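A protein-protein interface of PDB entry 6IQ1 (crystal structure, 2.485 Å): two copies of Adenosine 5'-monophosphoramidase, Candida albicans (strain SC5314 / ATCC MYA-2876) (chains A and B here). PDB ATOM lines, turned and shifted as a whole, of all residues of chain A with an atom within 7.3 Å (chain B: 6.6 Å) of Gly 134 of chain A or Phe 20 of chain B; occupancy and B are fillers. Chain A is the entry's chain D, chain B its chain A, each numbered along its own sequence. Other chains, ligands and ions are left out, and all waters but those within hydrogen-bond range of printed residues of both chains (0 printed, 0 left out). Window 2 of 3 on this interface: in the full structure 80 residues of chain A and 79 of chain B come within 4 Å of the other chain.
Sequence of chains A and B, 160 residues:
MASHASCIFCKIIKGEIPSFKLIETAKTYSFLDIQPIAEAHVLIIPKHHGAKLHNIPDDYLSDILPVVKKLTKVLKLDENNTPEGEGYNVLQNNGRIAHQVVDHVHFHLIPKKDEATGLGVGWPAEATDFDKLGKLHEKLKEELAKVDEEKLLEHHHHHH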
ATOM      1  N   THR A 128     -30.895  24.641  20.705  1.00  0.00           N
ATOM      2  CA  THR A 128     -30.233  23.380  20.999  1.00  0.00           C
ATOM      3  C   THR A 128     -30.859  22.718  22.219  1.00  0.00           C
ATOM      4  O   THR A 128     -31.752  23.260  22.884  1.00  0.00           O
ATOM      5  CB  THR A 128     -28.725  23.555  21.217  1.00  0.00           C
ATOM      6  OG1 THR A 128     -28.083  22.272  21.136  1.00  0.00           O
ATOM      7  CG2 THR A 128     -28.451  24.157  22.597  1.00  0.00           C
ATOM      8  N   ASP A 129     -30.300  21.564  22.556  1.00  0.00           N
ATOM      9  CA  ASP A 129     -30.953  20.575  23.391  1.00  0.00           C
ATOM     10  C   ASP A 129     -29.899  19.787  24.144  1.00  0.00           C
ATOM     11  O   ASP A 129     -28.798  19.586  23.626  1.00  0.00           O
ATOM     12  CB  ASP A 129     -31.737  19.654  22.462  1.00  0.00           C
ATOM     13  CG  ASP A 129     -33.033  19.267  23.014  1.00  0.00           C
ATOM     14  OD1 ASP A 129     -33.363  19.804  24.090  1.00  0.00           O
ATOM     15  OD2 ASP A 129     -33.707  18.408  22.391  1.00  0.00           O
ATOM     16  N   PHE A 130     -30.255  19.268  25.321  1.00  0.00           N
ATOM     17  CA  PHE A 130     -29.291  18.427  26.025  1.00  0.00           C
ATOM     18  C   PHE A 130     -29.094  17.088  25.318  1.00  0.00           C
ATOM     19  O   PHE A 130     -28.012  16.505  25.407  1.00  0.00           O
ATOM     20  CB  PHE A 130     -29.718  18.215  27.470  1.00  0.00           C
ATOM     21  CG  PHE A 130     -29.318  19.323  28.395  1.00  0.00           C
ATOM     22  CD1 PHE A 130     -28.091  19.936  28.277  1.00  0.00           C
ATOM     23  CD2 PHE A 130     -30.182  19.750  29.396  1.00  0.00           C
ATOM     24  CE1 PHE A 130     -27.722  20.981  29.133  1.00  0.00           C
ATOM     25  CE2 PHE A 130     -29.830  20.780  30.265  1.00  0.00           C
ATOM     26  CZ  PHE A 130     -28.592  21.403  30.128  1.00  0.00           C
ATOM     27  N   ASP A 131     -30.108  16.594  24.596  1.00  0.00           N
ATOM     28  CA  ASP A 131     -29.899  15.419  23.752  1.00  0.00           C
ATOM     29  C   ASP A 131     -28.872  15.709  22.667  1.00  0.00           C
ATOM     30  O   ASP A 131     -27.928  14.937  22.472  1.00  0.00           O
ATOM     31  CB  ASP A 131     -31.204  14.954  23.092  1.00  0.00           C
ATOM     32  CG  ASP A 131     -32.262  14.518  24.089  1.00  0.00           C
ATOM     33  OD1 ASP A 131     -31.909  14.015  25.184  1.00  0.00           O
ATOM     34  OD2 ASP A 131     -33.467  14.674  23.763  1.00  0.00           O
ATOM     35  N   LYS A 132     -29.067  16.810  21.927  1.00  0.00           N
ATOM     36  CA  LYS A 132     -28.149  17.171  20.847  1.00  0.00           C
ATOM     37  C   LYS A 132     -26.761  17.498  21.381  1.00  0.00           C
ATOM     38  O   LYS A 132     -25.758  17.069  20.802  1.00  0.00           O
ATOM     39  CB  LYS A 132     -28.704  18.347  20.049  1.00  0.00           C
ATOM     40  CG  LYS A 132     -29.762  17.936  19.054  1.00  0.00           C
ATOM     41  CD  LYS A 132     -30.679  19.089  18.689  1.00  0.00           C
ATOM     42  CE  LYS A 132     -31.911  18.573  17.955  1.00  0.00           C
ATOM     43  NZ  LYS A 132     -32.744  19.700  17.446  1.00  0.00           N
ATOM     44  N   LEU A 133     -26.678  18.234  22.494  1.00  0.00           N
ATOM     45  CA  LEU A 133     -25.374  18.507  23.090  1.00  0.00           C
ATOM     46  C   LEU A 133     -24.691  17.220  23.523  1.00  0.00           C
ATOM     47  O   LEU A 133     -23.487  17.044  23.292  1.00  0.00           O
ATOM     48  CB  LEU A 133     -25.518  19.469  24.267  1.00  0.00           C
ATOM     49  CG  LEU A 133     -25.846  20.899  23.825  1.00  0.00           C
ATOM     50  CD1 LEU A 133     -26.321  21.761  24.993  1.00  0.00           C
ATOM     51  CD2 LEU A 133     -24.639  21.521  23.132  1.00  0.00           C
ATOM     52  N   GLY A 134     -25.456  16.295  24.115  1.00  0.00           N
ATOM     53  CA  GLY A 134     -24.878  15.041  24.585  1.00  0.00           C
ATOM     54  C   GLY A 134     -24.336  14.175  23.460  1.00  0.00           C
ATOM     55  O   GLY A 134     -23.246  13.612  23.569  1.00  0.00           O
ATOM     56  N   LYS A 135     -25.095  14.048  22.361  1.00  0.00           N
ATOM     57  CA  LYS A 135     -24.623  13.232  21.247  1.00  0.00           C
ATOM     58  C   LYS A 135     -23.458  13.900  20.544  1.00  0.00           C
ATOM     59  O   LYS A 135     -22.520  13.224  20.101  1.00  0.00           O
ATOM     60  CB  LYS A 135     -25.758  12.948  20.258  1.00  0.00           C
ATOM     61  CG  LYS A 135     -27.076  12.546  20.944  1.00  0.00           C
ATOM     62  CD  LYS A 135     -28.219  12.245  19.974  1.00  0.00           C
ATOM     63  CE  LYS A 135     -29.407  11.524  20.669  1.00  0.00           C
ATOM     64  NZ  LYS A 135     -30.538  12.450  21.089  1.00  0.00           N
ATOM     65  N   LEU A 136     -23.482  15.226  20.463  1.00  0.00           N
ATOM     66  CA  LEU A 136     -22.333  15.944  19.937  1.00  0.00           C
ATOM     67  C   LEU A 136     -21.122  15.753  20.842  1.00  0.00           C
ATOM     68  O   LEU A 136     -19.985  15.619  20.367  1.00  0.00           O
ATOM     69  CB  LEU A 136     -22.681  17.426  19.796  1.00  0.00           C
ATOM     70  CG  LEU A 136     -21.498  18.316  19.426  1.00  0.00           C
ATOM     71  CD1 LEU A 136     -20.977  18.003  18.013  1.00  0.00           C
ATOM     72  CD2 LEU A 136     -21.900  19.758  19.564  1.00  0.00           C
ATOM     73  N   HIS A 137     -21.354  15.728  22.157  1.00  0.00           N
ATOM     74  CA  HIS A 137     -20.254  15.602  23.095  1.00  0.00           C
ATOM     75  C   HIS A 137     -19.620  14.221  23.029  1.00  0.00           C
ATOM     76  O   HIS A 137     -18.403  14.083  23.231  1.00  0.00           O
ATOM     77  CB  HIS A 137     -20.744  15.887  24.507  1.00  0.00           C
ATOM     78  CG  HIS A 137     -19.722  15.613  25.562  1.00  0.00           C
ATOM     79  ND1 HIS A 137     -19.805  14.535  26.415  1.00  0.00           N
ATOM     80  CD2 HIS A 137     -18.594  16.278  25.902  1.00  0.00           C
ATOM     81  CE1 HIS A 137     -18.774  14.554  27.240  1.00  0.00           C
ATOM     82  NE2 HIS A 137     -18.023  15.599  26.947  1.00  0.00           N
ATOM     83  N   GLU A 138     -20.425  13.188  22.769  1.00  0.00           N
ATOM     84  CA  GLU A 138     -19.864  11.852  22.616  1.00  0.00           C
ATOM     85  C   GLU A 138     -19.057  11.756  21.326  1.00  0.00           C
ATOM     86  O   GLU A 138     -17.993  11.125  21.300  1.00  0.00           O
ATOM     87  CB  GLU A 138     -20.976  10.806  22.658  1.00  0.00           C
ATOM     88  CG  GLU A 138     -20.495   9.375  22.473  1.00  0.00           C
ATOM     89  CD  GLU A 138     -21.606   8.426  22.039  1.00  0.00           C
ATOM     90  OE1 GLU A 138     -22.798   8.771  22.213  1.00  0.00           O
ATOM     91  OE2 GLU A 138     -21.286   7.337  21.511  1.00  0.00           O
ATOM     92  N   LYS A 139     -19.523  12.410  20.257  1.00  0.00           N
ATOM     93  CA  LYS A 139     -18.794  12.364  18.997  1.00  0.00           C
ATOM     94  C   LYS A 139     -17.442  13.065  19.111  1.00  0.00           C
ATOM     95  O   LYS A 139     -16.436  12.569  18.594  1.00  0.00           O
ATOM     96  CB  LYS A 139     -19.636  12.983  17.882  1.00  0.00           C
ATOM     97  CG  LYS A 139     -18.819  13.369  16.648  1.00  0.00           C
ATOM     98  CD  LYS A 139     -19.673  13.921  15.511  1.00  0.00           C
ATOM     99  CE  LYS A 139     -18.770  14.556  14.447  1.00  0.00           C
ATOM    100  NZ  LYS A 139     -19.476  14.963  13.190  1.00  0.00           N
ATOM    101  N   LEU A 140     -17.393  14.209  19.801  1.00  0.00           N
ATOM    102  CA  LEU A 140     -16.127  14.923  19.959  1.00  0.00           C
ATOM    103  C   LEU A 140     -15.174  14.199  20.903  1.00  0.00           C
ATOM    104  O   LEU A 140     -13.954  14.268  20.722  1.00  0.00           O
ATOM    105  CB  LEU A 140     -16.384  16.338  20.460  1.00  0.00           C
ATOM    106  CG  LEU A 140     -17.199  17.214  19.520  1.00  0.00           C
ATOM    107  CD1 LEU A 140     -17.410  18.568  20.179  1.00  0.00           C
ATOM    108  CD2 LEU A 140     -16.505  17.346  18.167  1.00  0.00           C
ATOM    109  N   PRO B  18     -22.567  20.844  36.223  1.00  0.00           N
ATOM    110  CA  PRO B  18     -22.081  19.926  35.186  1.00  0.00           C
ATOM    111  C   PRO B  18     -21.692  20.676  33.919  1.00  0.00           C
ATOM    112  O   PRO B  18     -22.095  21.819  33.682  1.00  0.00           O
ATOM    113  CB  PRO B  18     -23.271  18.992  34.932  1.00  0.00           C
ATOM    114  CG  PRO B  18     -24.237  19.216  36.088  1.00  0.00           C
ATOM    115  CD  PRO B  18     -23.987  20.623  36.564  1.00  0.00           C
ATOM    116  N   SER B  19     -20.885  20.011  33.098  1.00  0.00           N
ATOM    117  CA  SER B  19     -20.470  20.587  31.827  1.00  0.00           C
ATOM    118  C   SER B  19     -20.112  19.463  30.880  1.00  0.00           C
ATOM    119  O   SER B  19     -19.738  18.369  31.305  1.00  0.00           O
ATOM    120  CB  SER B  19     -19.276  21.528  31.977  1.00  0.00           C
ATOM    121  OG  SER B  19     -18.192  20.836  32.581  1.00  0.00           O
ATOM    122  N   PHE B  20     -20.247  19.746  29.589  1.00  0.00           N
ATOM    123  CA  PHE B  20     -19.856  18.801  28.555  1.00  0.00           C
ATOM    124  C   PHE B  20     -18.370  19.035  28.318  1.00  0.00           C
ATOM    125  O   PHE B  20     -17.949  19.778  27.424  1.00  0.00           O
ATOM    126  CB  PHE B  20     -20.693  19.001  27.299  1.00  0.00           C
ATOM    127  CG  PHE B  20     -22.156  18.656  27.470  1.00  0.00           C
ATOM    128  CD1 PHE B  20     -22.576  17.327  27.498  1.00  0.00           C
ATOM    129  CD2 PHE B  20     -23.113  19.659  27.574  1.00  0.00           C
ATOM    130  CE1 PHE B  20     -23.933  17.007  27.635  1.00  0.00           C
ATOM    131  CE2 PHE B  20     -24.475  19.346  27.716  1.00  0.00           C
ATOM    132  CZ  PHE B  20     -24.879  18.017  27.745  1.00  0.00           C
ATOM    133  N   LYS B  21     -17.563  18.394  29.159  1.00  0.00           N
ATOM    134  CA  LYS B  21     -16.136  18.662  29.196  1.00  0.00           C
ATOM    135  C   LYS B  21     -15.439  18.068  27.982  1.00  0.00           C
ATOM    136  O   LYS B  21     -15.763  16.963  27.539  1.00  0.00           O
ATOM    137  CB  LYS B  21     -15.550  18.094  30.484  1.00  0.00           C
ATOM    138  CG  LYS B  21     -14.215  18.660  30.879  1.00  0.00           C
ATOM    139  CD  LYS B  21     -13.639  17.867  32.025  1.00  0.00           C
ATOM    140  CE  LYS B  21     -13.393  16.432  31.606  1.00  0.00           C
ATOM    141  NZ  LYS B  21     -12.321  15.825  32.428  1.00  0.00           N
ATOM    142  N   LEU B  22     -14.471  18.815  27.441  1.00  0.00           N
ATOM    143  CA  LEU B  22     -13.723  18.377  26.272  1.00  0.00           C
ATOM    144  C   LEU B  22     -12.276  18.171  26.678  1.00  0.00           C
ATOM    145  O   LEU B  22     -11.939  17.116  27.255  1.00  0.00           O
ATOM    146  CB  LEU B  22     -13.892  19.390  25.134  1.00  0.00           C
ATOM    147  CG  LEU B  22     -15.286  19.349  24.528  1.00  0.00           C
ATOM    148  CD1 LEU B  22     -15.398  20.385  23.458  1.00  0.00           C
ATOM    149  CD2 LEU B  22     -15.577  17.949  23.994  1.00  0.00           C
ATOM    150  N   TYR B  29      -9.376  24.498  31.048  1.00  0.00           N
ATOM    151  CA  TYR B  29     -10.614  23.721  31.043  1.00  0.00           C
ATOM    152  C   TYR B  29     -11.484  24.132  29.858  1.00  0.00           C
ATOM    153  O   TYR B  29     -11.727  25.326  29.646  1.00  0.00           O
ATOM    154  CB  TYR B  29     -11.367  23.936  32.356  1.00  0.00           C
ATOM    155  CG  TYR B  29     -12.455  22.926  32.623  1.00  0.00           C
ATOM    156  CD1 TYR B  29     -13.715  23.061  32.049  1.00  0.00           C
ATOM    157  CD2 TYR B  29     -12.226  21.845  33.468  1.00  0.00           C
ATOM    158  CE1 TYR B  29     -14.715  22.145  32.300  1.00  0.00           C
ATOM    159  CE2 TYR B  29     -13.216  20.925  33.731  1.00  0.00           C
ATOM    160  CZ  TYR B  29     -14.460  21.079  33.149  1.00  0.00           C
ATOM    161  OH  TYR B  29     -15.442  20.160  33.409  1.00  0.00           O
ATOM    162  N   SER B  30     -11.977  23.161  29.098  1.00  0.00           N
ATOM    163  CA  SER B  30     -12.798  23.478  27.937  1.00  0.00           C
ATOM    164  C   SER B  30     -14.052  22.612  27.909  1.00  0.00           C
ATOM    165  O   SER B  30     -14.051  21.466  28.371  1.00  0.00           O
ATOM    166  CB  SER B  30     -12.002  23.315  26.619  1.00  0.00           C
ATOM    167  OG  SER B  30     -11.572  21.981  26.457  1.00  0.00           O
ATOM    168  N   PHE B  31     -15.121  23.167  27.347  1.00  0.00           N
ATOM    169  CA  PHE B  31     -16.408  22.487  27.348  1.00  0.00           C
ATOM    170  C   PHE B  31     -17.326  23.124  26.304  1.00  0.00           C
ATOM    171  O   PHE B  31     -17.126  24.273  25.884  1.00  0.00           O
ATOM    172  CB  PHE B  31     -17.051  22.533  28.736  1.00  0.00           C
ATOM    173  CG  PHE B  31     -17.197  23.922  29.291  1.00  0.00           C
ATOM    174  CD1 PHE B  31     -16.140  24.535  29.961  1.00  0.00           C
ATOM    175  CD2 PHE B  31     -18.389  24.626  29.142  1.00  0.00           C
ATOM    176  CE1 PHE B  31     -16.267  25.824  30.476  1.00  0.00           C
ATOM    177  CE2 PHE B  31     -18.519  25.908  29.663  1.00  0.00           C
ATOM    178  CZ  PHE B  31     -17.457  26.507  30.329  1.00  0.00           C
ATOM    179  N   LEU B  32     -18.338  22.352  25.894  1.00  0.00           N
ATOM    180  CA  LEU B  32     -19.334  22.844  24.947  1.00  0.00           C
ATOM    181  C   LEU B  32     -20.116  24.013  25.532  1.00  0.00           C
ATOM    182  O   LEU B  32     -20.521  23.996  26.694  1.00  0.00           O
ATOM    183  CB  LEU B  32     -20.309  21.732  24.565  1.00  0.00           C
ATOM    184  CG  LEU B  32     -19.730  20.596  23.725  1.00  0.00           C
ATOM    185  CD1 LEU B  32     -20.810  19.549  23.461  1.00  0.00           C
ATOM    186  CD2 LEU B  32     -19.158  21.134  22.413  1.00  0.00           C
ATOM    187  N   ASP B  33     -20.325  25.038  24.717  1.00  0.00           N
ATOM    188  CA  ASP B  33     -21.216  26.120  25.095  1.00  0.00           C
ATOM    189  C   ASP B  33     -22.648  25.604  25.023  1.00  0.00           C
ATOM    190  O   ASP B  33     -23.070  25.088  23.984  1.00  0.00           O
ATOM    191  CB  ASP B  33     -21.012  27.317  24.170  1.00  0.00           C
ATOM    192  CG  ASP B  33     -21.566  28.606  24.751  1.00  0.00           C
ATOM    193  OD1 ASP B  33     -22.545  28.551  25.530  1.00  0.00           O
ATOM    194  OD2 ASP B  33     -21.034  29.683  24.404  1.00  0.00           O
ATOM    195  N   ILE B  34     -23.383  25.692  26.138  1.00  0.00           N
ATOM    196  CA  ILE B  34     -24.757  25.198  26.140  1.00  0.00           C
ATOM    197  C   ILE B  34     -25.726  26.260  25.648  1.00  0.00           C
ATOM    198  O   ILE B  34     -26.923  25.981  25.522  1.00  0.00           O
ATOM    199  CB  ILE B  34     -25.210  24.647  27.515  1.00  0.00           C
ATOM    200  CG1 ILE B  34     -25.316  25.750  28.557  1.00  0.00           C
ATOM    201  CG2 ILE B  34     -24.296  23.495  28.001  1.00  0.00           C
ATOM    202  CD1 ILE B  34     -25.783  25.234  29.903  1.00  0.00           C
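Among the printed residues, pairs that only touch across the chains: Leu 133 of chain A with Phe 20 of chain B (3.6 Å), Leu 133 of chain A with Leu 32 of chain B (3.7 Å), His 137 of chain A with Phe 20 of chain B (3.7 Å), Phe 130 of chain A with Phe 20 of chain B (3.7 Å), Gly 134 of chain A with Phe 20 of chain B (3.7 Å), Thr 128 of chain A with Ile 34 of chain B (3.8 Å), His 137 of chain A with Leu 32 of chain B (3.8 Å), Leu 140 of chain A with Leu 32 of chain B (3.8 Å), His 137 of chain A with Leu 22 of chain B (3.9 Å), Leu 133 of chain A with Ile 34 of chain B (3.9 Å), Leu 140 of chain A with Leu 22 of chain B (3.97 Å) and Leu 133 of chain A with Asp 33 of chain B (3.99 Å).
Gly 134 of chain A touches just one residue of chain B: Phe 20 (3.7 Å). Of the printed residues of chain B, Thr 128 of chain A touches Ile 34 (3.8 Å). Printed residues of chain A within 4 Å of Lys 21 of chain B: His 137 (2.7 Å). Of the printed residues of chain B, Phe 130 of chain A touches Phe 20. Of the printed residues of chain B, His 137 of chain A touches Phe 20 (3.7 Å), Lys 21 (2.7 Å), Leu 22 (3.9 Å) and Leu 32 (3.8 Å). Printed residues of chain A within 4 Å of Ile 34 of chain B: Thr 128 and Leu 133. The nearest printed residue of chain B that does not touch Leu 133 of chain A is Leu 22 of chain B (8.0 Å).
Hydrophobic or aromatic side chains of chain A within 4 Å of the printed part of chain B: Phe 130, Leu 133, His 137 and Leu 140. Of the 11 printed residues of chain B, 6 touch a printed residue of chain A. Hydrophobic or aromatic side chains of chain B that line the printed part of chain A: Phe 20, Leu 22, Leu 32 and Ile 34. Among the printed residues, no Asp or Glu carboxylate lies within 4 Å of a Lys or Arg side-chain nitrogen of the other chain.
O of Phe 20 of chain B sits at hydrogen-bond distance from N of Leu 32 of chain B (3.0 Å). The backbone NH (N) of Leu 22 of chain B is in hydrogen-bond range of the backbone carbonyl oxygen (O) of Ser 30 of chain B.
No position is printed for both chains. Of the 13 pairs that touch across the chains among the printed residues, none has its exchanged pair printed and touching as well.
O of Lys 21 of chain B is in hydrogen-bond range of NE2 of His 137 of chain A (2.7 Å).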
